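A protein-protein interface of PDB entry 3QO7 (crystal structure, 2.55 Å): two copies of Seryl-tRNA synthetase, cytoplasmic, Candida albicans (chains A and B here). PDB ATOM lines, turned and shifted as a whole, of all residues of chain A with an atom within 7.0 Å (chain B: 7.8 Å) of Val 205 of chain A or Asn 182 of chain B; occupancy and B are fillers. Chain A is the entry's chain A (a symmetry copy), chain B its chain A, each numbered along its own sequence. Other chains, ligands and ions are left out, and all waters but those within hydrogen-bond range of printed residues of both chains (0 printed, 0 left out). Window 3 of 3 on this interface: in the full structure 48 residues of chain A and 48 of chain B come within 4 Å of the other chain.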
ATOM      1  N   LEU A 196     -14.150   7.926  -2.120  1.00  0.00           N
ATOM      2  CA  LEU A 196     -13.406   6.816  -1.486  1.00  0.00           C
ATOM      3  C   LEU A 196     -12.194   6.394  -2.313  1.00  0.00           C
ATOM      4  O   LEU A 196     -11.098   6.186  -1.788  1.00  0.00           O
ATOM      5  CB  LEU A 196     -14.316   5.616  -1.257  1.00  0.00           C
ATOM      6  CG  LEU A 196     -15.269   5.833  -0.079  1.00  0.00           C
ATOM      7  CD1 LEU A 196     -16.279   4.708   0.007  1.00  0.00           C
ATOM      8  CD2 LEU A 196     -14.492   5.967   1.248  1.00  0.00           C
ATOM      9  N   LEU A 199      -9.417   9.223  -2.356  1.00  0.00           N
ATOM     10  CA  LEU A 199      -8.647   9.398  -1.139  1.00  0.00           C
ATOM     11  C   LEU A 199      -7.771   8.176  -0.949  1.00  0.00           C
ATOM     12  O   LEU A 199      -6.603   8.262  -0.533  1.00  0.00           O
ATOM     13  CB  LEU A 199      -9.565   9.582   0.050  1.00  0.00           C
ATOM     14  CG  LEU A 199     -10.192  10.967   0.192  1.00  0.00           C
ATOM     15  CD1 LEU A 199     -10.971  11.031   1.488  1.00  0.00           C
ATOM     16  CD2 LEU A 199      -9.125  12.064   0.175  1.00  0.00           C
ATOM     17  N   SER A 200      -8.334   7.029  -1.291  1.00  0.00           N
ATOM     18  CA  SER A 200      -7.621   5.793  -1.098  1.00  0.00           C
ATOM     19  C   SER A 200      -6.347   5.742  -1.979  1.00  0.00           C
ATOM     20  O   SER A 200      -5.283   5.298  -1.536  1.00  0.00           O
ATOM     21  CB  SER A 200      -8.559   4.613  -1.311  1.00  0.00           C
ATOM     22  OG  SER A 200      -7.861   3.558  -1.912  1.00  0.00           O
ATOM     23  N   LYS A 202      -4.570   8.146  -2.508  1.00  0.00           N
ATOM     24  CA  LYS A 202      -3.620   8.981  -1.792  1.00  0.00           C
ATOM     25  C   LYS A 202      -3.232   8.368  -0.435  1.00  0.00           C
ATOM     26  O   LYS A 202      -2.713   9.052   0.447  1.00  0.00           O
ATOM     27  CB  LYS A 202      -4.200  10.371  -1.595  1.00  0.00           C
ATOM     28  CG  LYS A 202      -4.416  11.091  -2.886  1.00  0.00           C
ATOM     29  CD  LYS A 202      -5.005  12.478  -2.672  1.00  0.00           C
ATOM     30  CE  LYS A 202      -4.179  13.530  -3.403  1.00  0.00           C
ATOM     31  NZ  LYS A 202      -4.266  13.328  -4.869  1.00  0.00           N
ATOM     32  N   GLY A 203      -3.495   7.080  -0.266  1.00  0.00           N
ATOM     33  CA  GLY A 203      -3.088   6.395   0.943  1.00  0.00           C
ATOM     34  C   GLY A 203      -3.998   6.540   2.148  1.00  0.00           C
ATOM     35  O   GLY A 203      -3.615   6.102   3.234  1.00  0.00           O
ATOM     36  N   TYR A 204      -5.176   7.150   1.980  1.00  0.00           N
ATOM     37  CA  TYR A 204      -6.175   7.183   3.039  1.00  0.00           C
ATOM     38  C   TYR A 204      -6.811   5.807   3.175  1.00  0.00           C
ATOM     39  O   TYR A 204      -7.011   5.106   2.176  1.00  0.00           O
ATOM     40  CB  TYR A 204      -7.287   8.164   2.709  1.00  0.00           C
ATOM     41  CG  TYR A 204      -6.892   9.601   2.828  1.00  0.00           C
ATOM     42  CD1 TYR A 204      -7.476  10.430   3.792  1.00  0.00           C
ATOM     43  CD2 TYR A 204      -5.925  10.133   1.986  1.00  0.00           C
ATOM     44  CE1 TYR A 204      -7.093  11.772   3.909  1.00  0.00           C
ATOM     45  CE2 TYR A 204      -5.535  11.445   2.080  1.00  0.00           C
ATOM     46  CZ  TYR A 204      -6.117  12.273   3.040  1.00  0.00           C
ATOM     47  OH  TYR A 204      -5.706  13.597   3.101  1.00  0.00           O
ATOM     48  N   VAL A 205      -7.143   5.428   4.406  1.00  0.00           N
ATOM     49  CA  VAL A 205      -7.783   4.149   4.663  1.00  0.00           C
ATOM     50  C   VAL A 205      -9.304   4.338   4.722  1.00  0.00           C
ATOM     51  O   VAL A 205      -9.801   5.037   5.603  1.00  0.00           O
ATOM     52  CB  VAL A 205      -7.279   3.587   6.009  1.00  0.00           C
ATOM     53  CG1 VAL A 205      -8.136   2.393   6.487  1.00  0.00           C
ATOM     54  CG2 VAL A 205      -5.796   3.230   5.914  1.00  0.00           C
ATOM     55  N   PRO A 206     -10.051   3.725   3.780  1.00  0.00           N
ATOM     56  CA  PRO A 206     -11.514   3.847   3.818  1.00  0.00           C
ATOM     57  C   PRO A 206     -12.005   3.365   5.159  1.00  0.00           C
ATOM     58  O   PRO A 206     -11.491   2.358   5.670  1.00  0.00           O
ATOM     59  CB  PRO A 206     -11.980   2.880   2.725  1.00  0.00           C
ATOM     60  CG  PRO A 206     -10.868   2.861   1.759  1.00  0.00           C
ATOM     61  CD  PRO A 206      -9.601   2.952   2.612  1.00  0.00           C
ATOM     62  N   LEU A 207     -12.982   4.061   5.723  1.00  0.00           N
ATOM     63  CA  LEU A 207     -13.439   3.749   7.069  1.00  0.00           C
ATOM     64  C   LEU A 207     -14.891   4.168   7.215  1.00  0.00           C
ATOM     65  O   LEU A 207     -15.171   5.366   7.260  1.00  0.00           O
ATOM     66  CB  LEU A 207     -12.584   4.513   8.083  1.00  0.00           C
ATOM     67  CG  LEU A 207     -12.798   4.109   9.536  1.00  0.00           C
ATOM     68  CD1 LEU A 207     -12.409   2.627   9.704  1.00  0.00           C
ATOM     69  CD2 LEU A 207     -11.968   5.000  10.460  1.00  0.00           C
ATOM     70  N   GLN A 208     -15.818   3.213   7.257  1.00  0.00           N
ATOM     71  CA  GLN A 208     -17.236   3.537   7.388  1.00  0.00           C
ATOM     72  C   GLN A 208     -17.597   3.582   8.836  1.00  0.00           C
ATOM     73  O   GLN A 208     -17.542   2.562   9.513  1.00  0.00           O
ATOM     74  CB  GLN A 208     -18.128   2.502   6.679  1.00  0.00           C
ATOM     75  CG  GLN A 208     -19.658   2.817   6.751  1.00  0.00           C
ATOM     76  CD  GLN A 208     -20.456   2.063   5.694  1.00  0.00           C
ATOM     77  OE1 GLN A 208     -19.947   1.747   4.596  1.00  0.00           O
ATOM     78  NE2 GLN A 208     -21.712   1.742   6.025  1.00  0.00           N
ATOM     79  N   TYR A 254     -11.769   7.012  17.367  1.00  0.00           N
ATOM     80  CA  TYR A 254     -11.347   5.695  16.910  1.00  0.00           C
ATOM     81  C   TYR A 254     -10.120   5.198  17.670  1.00  0.00           C
ATOM     82  O   TYR A 254     -10.055   4.034  18.062  1.00  0.00           O
ATOM     83  CB  TYR A 254     -11.065   5.747  15.407  1.00  0.00           C
ATOM     84  CG  TYR A 254     -10.857   4.422  14.729  1.00  0.00           C
ATOM     85  CD1 TYR A 254     -11.919   3.539  14.541  1.00  0.00           C
ATOM     86  CD2 TYR A 254      -9.605   4.059  14.241  1.00  0.00           C
ATOM     87  CE1 TYR A 254     -11.743   2.320  13.879  1.00  0.00           C
ATOM     88  CE2 TYR A 254      -9.418   2.849  13.576  1.00  0.00           C
ATOM     89  CZ  TYR A 254     -10.496   1.982  13.403  1.00  0.00           C
ATOM     90  OH  TYR A 254     -10.319   0.778  12.764  1.00  0.00           O
ATOM     91  N   VAL A 269      -1.554   8.916  10.240  1.00  0.00           N
ATOM     92  CA  VAL A 269      -2.609   7.984   9.906  1.00  0.00           C
ATOM     93  C   VAL A 269      -3.705   8.751   9.179  1.00  0.00           C
ATOM     94  O   VAL A 269      -4.171   9.777   9.661  1.00  0.00           O
ATOM     95  CB  VAL A 269      -3.151   7.322  11.170  1.00  0.00           C
ATOM     96  CG1 VAL A 269      -4.423   6.570  10.871  1.00  0.00           C
ATOM     97  CG2 VAL A 269      -2.094   6.380  11.754  1.00  0.00           C
ATOM     98  N   ARG A 270      -4.107   8.279   8.005  1.00  0.00           N
ATOM     99  CA  ARG A 270      -5.111   9.018   7.244  1.00  0.00           C
ATOM    100  C   ARG A 270      -6.362   8.199   6.958  1.00  0.00           C
ATOM    101  O   ARG A 270      -6.284   7.097   6.398  1.00  0.00           O
ATOM    102  CB  ARG A 270      -4.502   9.521   5.948  1.00  0.00           C
ATOM    103  CG  ARG A 270      -3.234  10.395   6.144  1.00  0.00           C
ATOM    104  CD  ARG A 270      -2.836  11.075   4.823  1.00  0.00           C
ATOM    105  NE  ARG A 270      -1.703  11.989   4.938  1.00  0.00           N
ATOM    106  CZ  ARG A 270      -0.468  11.706   4.527  1.00  0.00           C
ATOM    107  NH1 ARG A 270      -0.206  10.519   3.988  1.00  0.00           N
ATOM    108  NH2 ARG A 270       0.507  12.597   4.662  1.00  0.00           N
ATOM    109  N   TYR A 271      -7.522   8.733   7.331  1.00  0.00           N
ATOM    110  CA  TYR A 271      -8.775   8.010   7.102  1.00  0.00           C
ATOM    111  C   TYR A 271      -9.683   8.720   6.114  1.00  0.00           C
ATOM    112  O   TYR A 271      -9.868   9.931   6.211  1.00  0.00           O
ATOM    113  CB  TYR A 271      -9.534   7.800   8.400  1.00  0.00           C
ATOM    114  CG  TYR A 271      -8.817   6.883   9.335  1.00  0.00           C
ATOM    115  CD1 TYR A 271      -8.579   5.560   8.983  1.00  0.00           C
ATOM    116  CD2 TYR A 271      -8.348   7.335  10.565  1.00  0.00           C
ATOM    117  CE1 TYR A 271      -7.908   4.716   9.826  1.00  0.00           C
ATOM    118  CE2 TYR A 271      -7.679   6.486  11.425  1.00  0.00           C
ATOM    119  CZ  TYR A 271      -7.459   5.182  11.055  1.00  0.00           C
ATOM    120  OH  TYR A 271      -6.785   4.335  11.897  1.00  0.00           O
ATOM    121  N   ALA A 272     -10.240   7.951   5.179  1.00  0.00           N
ATOM    122  CA  ALA A 272     -11.289   8.434   4.292  1.00  0.00           C
ATOM    123  C   ALA A 272     -12.591   8.019   4.923  1.00  0.00           C
ATOM    124  O   ALA A 272     -13.082   6.917   4.657  1.00  0.00           O
ATOM    125  CB  ALA A 272     -11.155   7.811   2.888  1.00  0.00           C
ATOM    126  N   GLY A 273     -13.137   8.873   5.780  1.00  0.00           N
ATOM    127  CA  GLY A 273     -14.348   8.547   6.516  1.00  0.00           C
ATOM    128  C   GLY A 273     -15.564   8.640   5.609  1.00  0.00           C
ATOM    129  O   GLY A 273     -15.662   9.541   4.774  1.00  0.00           O
ATOM    130  N   LEU B 161      -8.903 -10.059   7.117  1.00  0.00           N
ATOM    131  CA  LEU B 161      -8.769  -9.138   5.979  1.00  0.00           C
ATOM    132  C   LEU B 161      -8.579  -7.703   6.460  1.00  0.00           C
ATOM    133  O   LEU B 161      -8.361  -6.783   5.667  1.00  0.00           O
ATOM    134  CB  LEU B 161      -9.998  -9.183   5.053  1.00  0.00           C
ATOM    135  CG  LEU B 161     -10.163 -10.435   4.182  1.00  0.00           C
ATOM    136  CD1 LEU B 161     -11.568 -10.526   3.589  1.00  0.00           C
ATOM    137  CD2 LEU B 161      -9.082 -10.497   3.102  1.00  0.00           C
ATOM    138  N   ASP B 162      -8.677  -7.523   7.768  1.00  0.00           N
ATOM    139  CA  ASP B 162      -8.700  -6.197   8.343  1.00  0.00           C
ATOM    140  C   ASP B 162      -9.833  -5.378   7.723  1.00  0.00           C
ATOM    141  O   ASP B 162      -9.667  -4.200   7.365  1.00  0.00           O
ATOM    142  CB  ASP B 162      -7.360  -5.511   8.162  1.00  0.00           C
ATOM    143  CG  ASP B 162      -7.204  -4.311   9.074  1.00  0.00           C
ATOM    144  OD1 ASP B 162      -8.013  -4.173  10.039  1.00  0.00           O
ATOM    145  OD2 ASP B 162      -6.267  -3.510   8.829  1.00  0.00           O
ATOM    146  N   GLY B 163     -11.003  -5.990   7.634  1.00  0.00           N
ATOM    147  CA  GLY B 163     -12.097  -5.370   6.928  1.00  0.00           C
ATOM    148  C   GLY B 163     -13.133  -4.779   7.851  1.00  0.00           C
ATOM    149  O   GLY B 163     -14.093  -4.140   7.405  1.00  0.00           O
ATOM    150  N   TYR B 164     -12.986  -5.012   9.148  1.00  0.00           N
ATOM    151  CA  TYR B 164     -13.924  -4.372  10.052  1.00  0.00           C
ATOM    152  C   TYR B 164     -13.326  -4.267  11.421  1.00  0.00           C
ATOM    153  O   TYR B 164     -12.303  -4.890  11.702  1.00  0.00           O
ATOM    154  CB  TYR B 164     -15.322  -5.035  10.053  1.00  0.00           C
ATOM    155  CG  TYR B 164     -15.568  -6.111  11.099  1.00  0.00           C
ATOM    156  CD1 TYR B 164     -16.739  -6.107  11.859  1.00  0.00           C
ATOM    157  CD2 TYR B 164     -14.658  -7.149  11.304  1.00  0.00           C
ATOM    158  CE1 TYR B 164     -16.991  -7.098  12.816  1.00  0.00           C
ATOM    159  CE2 TYR B 164     -14.904  -8.142  12.244  1.00  0.00           C
ATOM    160  CZ  TYR B 164     -16.071  -8.112  13.000  1.00  0.00           C
ATOM    161  OH  TYR B 164     -16.316  -9.095  13.936  1.00  0.00           O
ATOM    162  N   PHE B 179     -17.128  -0.496  12.826  1.00  0.00           N
ATOM    163  CA  PHE B 179     -16.708   0.230  11.637  1.00  0.00           C
ATOM    164  C   PHE B 179     -16.416  -0.788  10.554  1.00  0.00           C
ATOM    165  O   PHE B 179     -15.931  -1.876  10.846  1.00  0.00           O
ATOM    166  CB  PHE B 179     -15.396   0.957  11.875  1.00  0.00           C
ATOM    167  CG  PHE B 179     -15.465   2.066  12.874  1.00  0.00           C
ATOM    168  CD1 PHE B 179     -15.395   3.403  12.450  1.00  0.00           C
ATOM    169  CD2 PHE B 179     -15.559   1.784  14.239  1.00  0.00           C
ATOM    170  CE1 PHE B 179     -15.429   4.433  13.379  1.00  0.00           C
ATOM    171  CE2 PHE B 179     -15.602   2.813  15.174  1.00  0.00           C
ATOM    172  CZ  PHE B 179     -15.526   4.137  14.749  1.00  0.00           C
ATOM    173  N   LEU B 180     -16.673  -0.428   9.302  1.00  0.00           N
ATOM    174  CA  LEU B 180     -16.126  -1.190   8.179  1.00  0.00           C
ATOM    175  C   LEU B 180     -14.828  -0.515   7.779  1.00  0.00           C
ATOM    176  O   LEU B 180     -14.687   0.703   7.919  1.00  0.00           O
ATOM    177  CB  LEU B 180     -17.099  -1.261   7.001  1.00  0.00           C
ATOM    178  CG  LEU B 180     -18.360  -2.105   7.260  1.00  0.00           C
ATOM    179  CD1 LEU B 180     -19.392  -1.960   6.127  1.00  0.00           C
ATOM    180  CD2 LEU B 180     -17.963  -3.550   7.430  1.00  0.00           C
ATOM    181  N   ARG B 181     -13.873  -1.309   7.315  1.00  0.00           N
ATOM    182  CA  ARG B 181     -12.524  -0.827   7.086  1.00  0.00           C
ATOM    183  C   ARG B 181     -12.033  -1.381   5.745  1.00  0.00           C
ATOM    184  O   ARG B 181     -12.279  -2.556   5.403  1.00  0.00           O
ATOM    185  CB  ARG B 181     -11.627  -1.250   8.254  1.00  0.00           C
ATOM    186  CG  ARG B 181     -10.332  -0.491   8.386  1.00  0.00           C
ATOM    187  CD  ARG B 181      -9.380  -1.111   9.490  1.00  0.00           C
ATOM    188  NE  ARG B 181      -7.980  -0.770   9.207  1.00  0.00           N
ATOM    189  CZ  ARG B 181      -7.323   0.219   9.805  1.00  0.00           C
ATOM    190  NH1 ARG B 181      -7.936   0.931  10.750  1.00  0.00           N
ATOM    191  NH2 ARG B 181      -6.058   0.513   9.464  1.00  0.00           N
ATOM    192  N   ASN B 182     -11.396  -0.524   4.950  1.00  0.00           N
ATOM    193  CA  ASN B 182     -10.776  -0.990   3.728  1.00  0.00           C
ATOM    194  C   ASN B 182     -11.747  -1.727   2.836  1.00  0.00           C
ATOM    195  O   ASN B 182     -12.813  -1.227   2.472  1.00  0.00           O
ATOM    196  CB  ASN B 182      -9.678  -1.983   4.093  1.00  0.00           C
ATOM    197  CG  ASN B 182      -8.477  -1.314   4.668  1.00  0.00           C
ATOM    198  OD1 ASN B 182      -7.941  -0.402   4.044  1.00  0.00           O
ATOM    199  ND2 ASN B 182      -8.047  -1.737   5.872  1.00  0.00           N
ATOM    200  N   TYR B 183     -11.360  -2.951   2.500  1.00  0.00           N
ATOM    201  CA  TYR B 183     -12.152  -3.740   1.590  1.00  0.00           C
ATOM    202  C   TYR B 183     -13.541  -4.059   2.150  1.00  0.00           C
ATOM    203  O   TYR B 183     -14.460  -4.387   1.393  1.00  0.00           O
ATOM    204  CB  TYR B 183     -11.382  -4.984   1.181  1.00  0.00           C
ATOM    205  CG  TYR B 183     -10.341  -4.678   0.140  1.00  0.00           C
ATOM    206  CD1 TYR B 183     -10.716  -4.324  -1.163  1.00  0.00           C
ATOM    207  CD2 TYR B 183      -8.983  -4.730   0.444  1.00  0.00           C
ATOM    208  CE1 TYR B 183      -9.762  -4.025  -2.141  1.00  0.00           C
ATOM    209  CE2 TYR B 183      -8.014  -4.436  -0.529  1.00  0.00           C
ATOM    210  CZ  TYR B 183      -8.409  -4.082  -1.814  1.00  0.00           C
ATOM    211  OH  TYR B 183      -7.459  -3.803  -2.767  1.00  0.00           O
ATOM    212  N   GLY B 184     -13.698  -3.951   3.467  1.00  0.00           N
ATOM    213  CA  GLY B 184     -15.006  -4.145   4.063  1.00  0.00           C
ATOM    214  C   GLY B 184     -15.907  -3.030   3.552  1.00  0.00           C
ATOM    215  O   GLY B 184     -17.049  -3.274   3.157  1.00  0.00           O
ATOM    216  N   VAL B 185     -15.377  -1.808   3.525  1.00  0.00           N
ATOM    217  CA  VAL B 185     -16.078  -0.690   2.923  1.00  0.00           C
ATOM    218  C   VAL B 185     -16.362  -0.885   1.427  1.00  0.00           C
ATOM    219  O   VAL B 185     -17.487  -0.665   0.966  1.00  0.00           O
ATOM    220  CB  VAL B 185     -15.294   0.619   3.079  1.00  0.00           C
ATOM    221  CG1 VAL B 185     -16.056   1.751   2.396  1.00  0.00           C
ATOM    222  CG2 VAL B 185     -15.021   0.947   4.572  1.00  0.00           C
ATOM    223  N   PHE B 186     -15.354  -1.283   0.662  1.00  0.00           N
ATOM    224  CA  PHE B 186     -15.538  -1.479  -0.784  1.00  0.00           C
ATOM    225  C   PHE B 186     -16.521  -2.595  -1.112  1.00  0.00           C
ATOM    226  O   PHE B 186     -17.217  -2.534  -2.141  1.00  0.00           O
ATOM    227  CB  PHE B 186     -14.221  -1.807  -1.469  1.00  0.00           C
ATOM    228  CG  PHE B 186     -13.233  -0.692  -1.448  1.00  0.00           C
ATOM    229  CD1 PHE B 186     -13.613   0.594  -1.794  1.00  0.00           C
ATOM    230  CD2 PHE B 186     -11.911  -0.927  -1.086  1.00  0.00           C
ATOM    231  CE1 PHE B 186     -12.688   1.633  -1.793  1.00  0.00           C
ATOM    232  CE2 PHE B 186     -10.980   0.118  -1.068  1.00  0.00           C
ATOM    233  CZ  PHE B 186     -11.369   1.393  -1.427  1.00  0.00           C
ATOM    234  N   LEU B 187     -16.560  -3.634  -0.273  1.00  0.00           N
ATOM    235  CA  LEU B 187     -17.449  -4.751  -0.567  1.00  0.00           C
ATOM    236  C   LEU B 187     -18.868  -4.329  -0.309  1.00  0.00           C
ATOM    237  O   LEU B 187     -19.787  -4.732  -1.019  1.00  0.00           O
ATOM    238  CB  LEU B 187     -17.109  -5.996   0.248  1.00  0.00           C
ATOM    239  CG  LEU B 187     -16.036  -6.875  -0.401  1.00  0.00           C
ATOM    240  CD1 LEU B 187     -15.339  -7.702   0.638  1.00  0.00           C
ATOM    241  CD2 LEU B 187     -16.638  -7.744  -1.493  1.00  0.00           C
ATOM    242  N   ASN B 188     -19.041  -3.499   0.706  1.00  0.00           N
ATOM    243  CA  ASN B 188     -20.369  -3.049   1.030  1.00  0.00           C
ATOM    244  C   ASN B 188     -20.935  -2.141  -0.058  1.00  0.00           C
ATOM    245  O   ASN B 188     -22.079  -2.305  -0.483  1.00  0.00           O
ATOM    246  CB  ASN B 188     -20.394  -2.362   2.380  1.00  0.00           C
ATOM    247  CG  ASN B 188     -21.791  -2.320   2.947  1.00  0.00           C
ATOM    248  OD1 ASN B 188     -22.436  -3.367   3.137  1.00  0.00           O
ATOM    249  ND2 ASN B 188     -22.296  -1.116   3.179  1.00  0.00           N
ATOM    250  N   ILE B 435     -15.058  -2.218  -7.571  1.00  0.00           N
ATOM    251  CA  ILE B 435     -14.026  -2.096  -6.552  1.00  0.00           C
ATOM    252  C   ILE B 435     -12.755  -1.510  -7.137  1.00  0.00           C
ATOM    253  O   ILE B 435     -12.241  -2.010  -8.144  1.00  0.00           O
ATOM    254  CB  ILE B 435     -13.707  -3.475  -5.909  1.00  0.00           C
ATOM    255  CG1 ILE B 435     -14.960  -4.007  -5.184  1.00  0.00           C
ATOM    256  CG2 ILE B 435     -12.511  -3.347  -4.960  1.00  0.00           C
ATOM    257  CD1 ILE B 435     -14.827  -5.440  -4.597  1.00  0.00           C
ATOM    258  N   ILE B 442      -8.047 -10.854  -2.533  1.00  0.00           N
ATOM    259  CA  ILE B 442      -7.405 -10.025  -1.547  1.00  0.00           C
ATOM    260  C   ILE B 442      -6.847 -10.909  -0.451  1.00  0.00           C
ATOM    261  O   ILE B 442      -7.474 -11.870  -0.028  1.00  0.00           O
ATOM    262  CB  ILE B 442      -8.342  -8.948  -0.971  1.00  0.00           C
ATOM    263  CG1 ILE B 442      -9.573  -9.574  -0.328  1.00  0.00           C
ATOM    264  CG2 ILE B 442      -8.776  -7.976  -2.050  1.00  0.00           C
ATOM    265  CD1 ILE B 442     -10.462  -8.539   0.314  1.00  0.00           C
ATOM    266  N   ILE B 445      -4.428 -10.161   6.017  1.00  0.00           N
ATOM    267  CA  ILE B 445      -3.457  -9.172   6.465  1.00  0.00           C
ATOM    268  C   ILE B 445      -3.074  -9.513   7.891  1.00  0.00           C
ATOM    269  O   ILE B 445      -1.993  -9.164   8.358  1.00  0.00           O
ATOM    270  CB  ILE B 445      -4.096  -7.743   6.512  1.00  0.00           C
ATOM    271  CG1 ILE B 445      -4.588  -7.305   5.141  1.00  0.00           C
ATOM    272  CG2 ILE B 445      -3.117  -6.727   7.030  1.00  0.00           C
ATOM    273  CD1 ILE B 445      -3.523  -7.406   4.116  1.00  0.00           C
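The backbone NH (N) of Gln 208 of chain A sits at hydrogen-bond distance from the backbone carbonyl oxygen (O) of Leu 180 of chain B, at 2.8 Å.
NH1 of Arg 181 of chain B lies within hydrogen-bond range of OH of Tyr 254 of chain A.
O of Pro 206 of chain A lies within hydrogen-bond range of N of Asn 182 of chain B, 3.0 Å away.
The side-chain carboxylate (OD2) of Asp 162 of chain B is in salt-bridge range of the guanidinium group (NE) of Arg 181 of chain B, 3.3 Å away.
The side-chain amide nitrogen of Asn 182 of chain B sits at hydrogen-bond distance from the backbone carbonyl oxygen of Asp 162 of chain B (3.3 Å).
The backbone NH of Arg 181 of chain B is in hydrogen-bond range of the backbone carbonyl oxygen of Gly 163 of chain B (2.8 Å).
The backbone NH of Val 205 of chain A is in hydrogen-bond range of the backbone carbonyl oxygen of Arg 270 of chain A, 2.7 Å away.
The backbone carbonyl oxygen of Val 205 of chain A sits at hydrogen-bond distance from the backbone NH of Ala 272 of chain A, 3.0 Å away.
O of Ala 272 of chain A sits at hydrogen-bond distance from N of Leu 207 of chain A, 3.1 Å away.
Among the printed residues, pairs that only touch across the chains: Gln 208 of chain A with Phe 179 of chain B, Leu 207 of chain A with Leu 180 of chain B, Pro 206 of chain A with Phe 186 of chain B, Gln 208 of chain A with Val 185 of chain B, Pro 206 of chain A with Arg 181 of chain B, Tyr 254 of chain A with Phe 179 of chain B, Val 205 of chain A with Asn 182 of chain B, Tyr 271 of chain A with Arg 181 of chain B, Leu 196 of chain A with Val 185 of chain B, Leu 207 of chain A with Val 185 of chain B, Pro 206 of chain A with Val 185 of chain B, Gln 208 of chain A with Asn 188 of chain B, Leu 207 of chain A with Phe 179 of chain B and Leu 207 of chain A with Arg 181 of chain B.
Val 205 of chain A touches just one residue of chain B: Asn 182 (3.7 Å).
Of the printed residues of chain B, Pro 206 of chain A touches Arg 181, Asn 182, Val 185 and Phe 186.
Of the printed residues of chain A, Phe 186 of chain B touches Pro 206 (3.5 Å).
Of the printed residues of chain A, Val 185 of chain B touches Leu 196, Pro 206, Leu 207 and Gln 208.
Of the printed residues of chain B, Tyr 271 of chain A touches Arg 181 (3.8 Å).
Gly 203 of chain A touches none of the printed residues of chain B.
The nearest residue of chain B that does not touch Val 205 of chain A is Arg 181 of chain B (4.05 Å).
The nearest printed residue of chain A that does not touch Leu 180 of chain B is Pro 206 of chain A (4.2 Å).
Of the 17 printed residues of chain B, 7 touch a printed residue of chain A.
Printed residues of chain B that touch a printed residue of chain A: Phe 179, Leu 180, Arg 181, Asn 182, Val 185, Phe 186 and Asn 188.
Hydrophobic or aromatic side chains of chain B within 4 Å of the printed part of chain A: Phe 179, Leu 180, Val 185 and Phe 186.
Hydrophobic or aromatic side chains of chain A that line the printed part of chain B: Leu 196, Val 205, Pro 206, Leu 207, Tyr 254 and Tyr 271.
Among the printed residues, 17 pairs touch across the chains.
No position is printed for both chains.
Of the 17 pairs that touch across the chains among the printed residues, none has its exchanged pair printed and touching as well.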
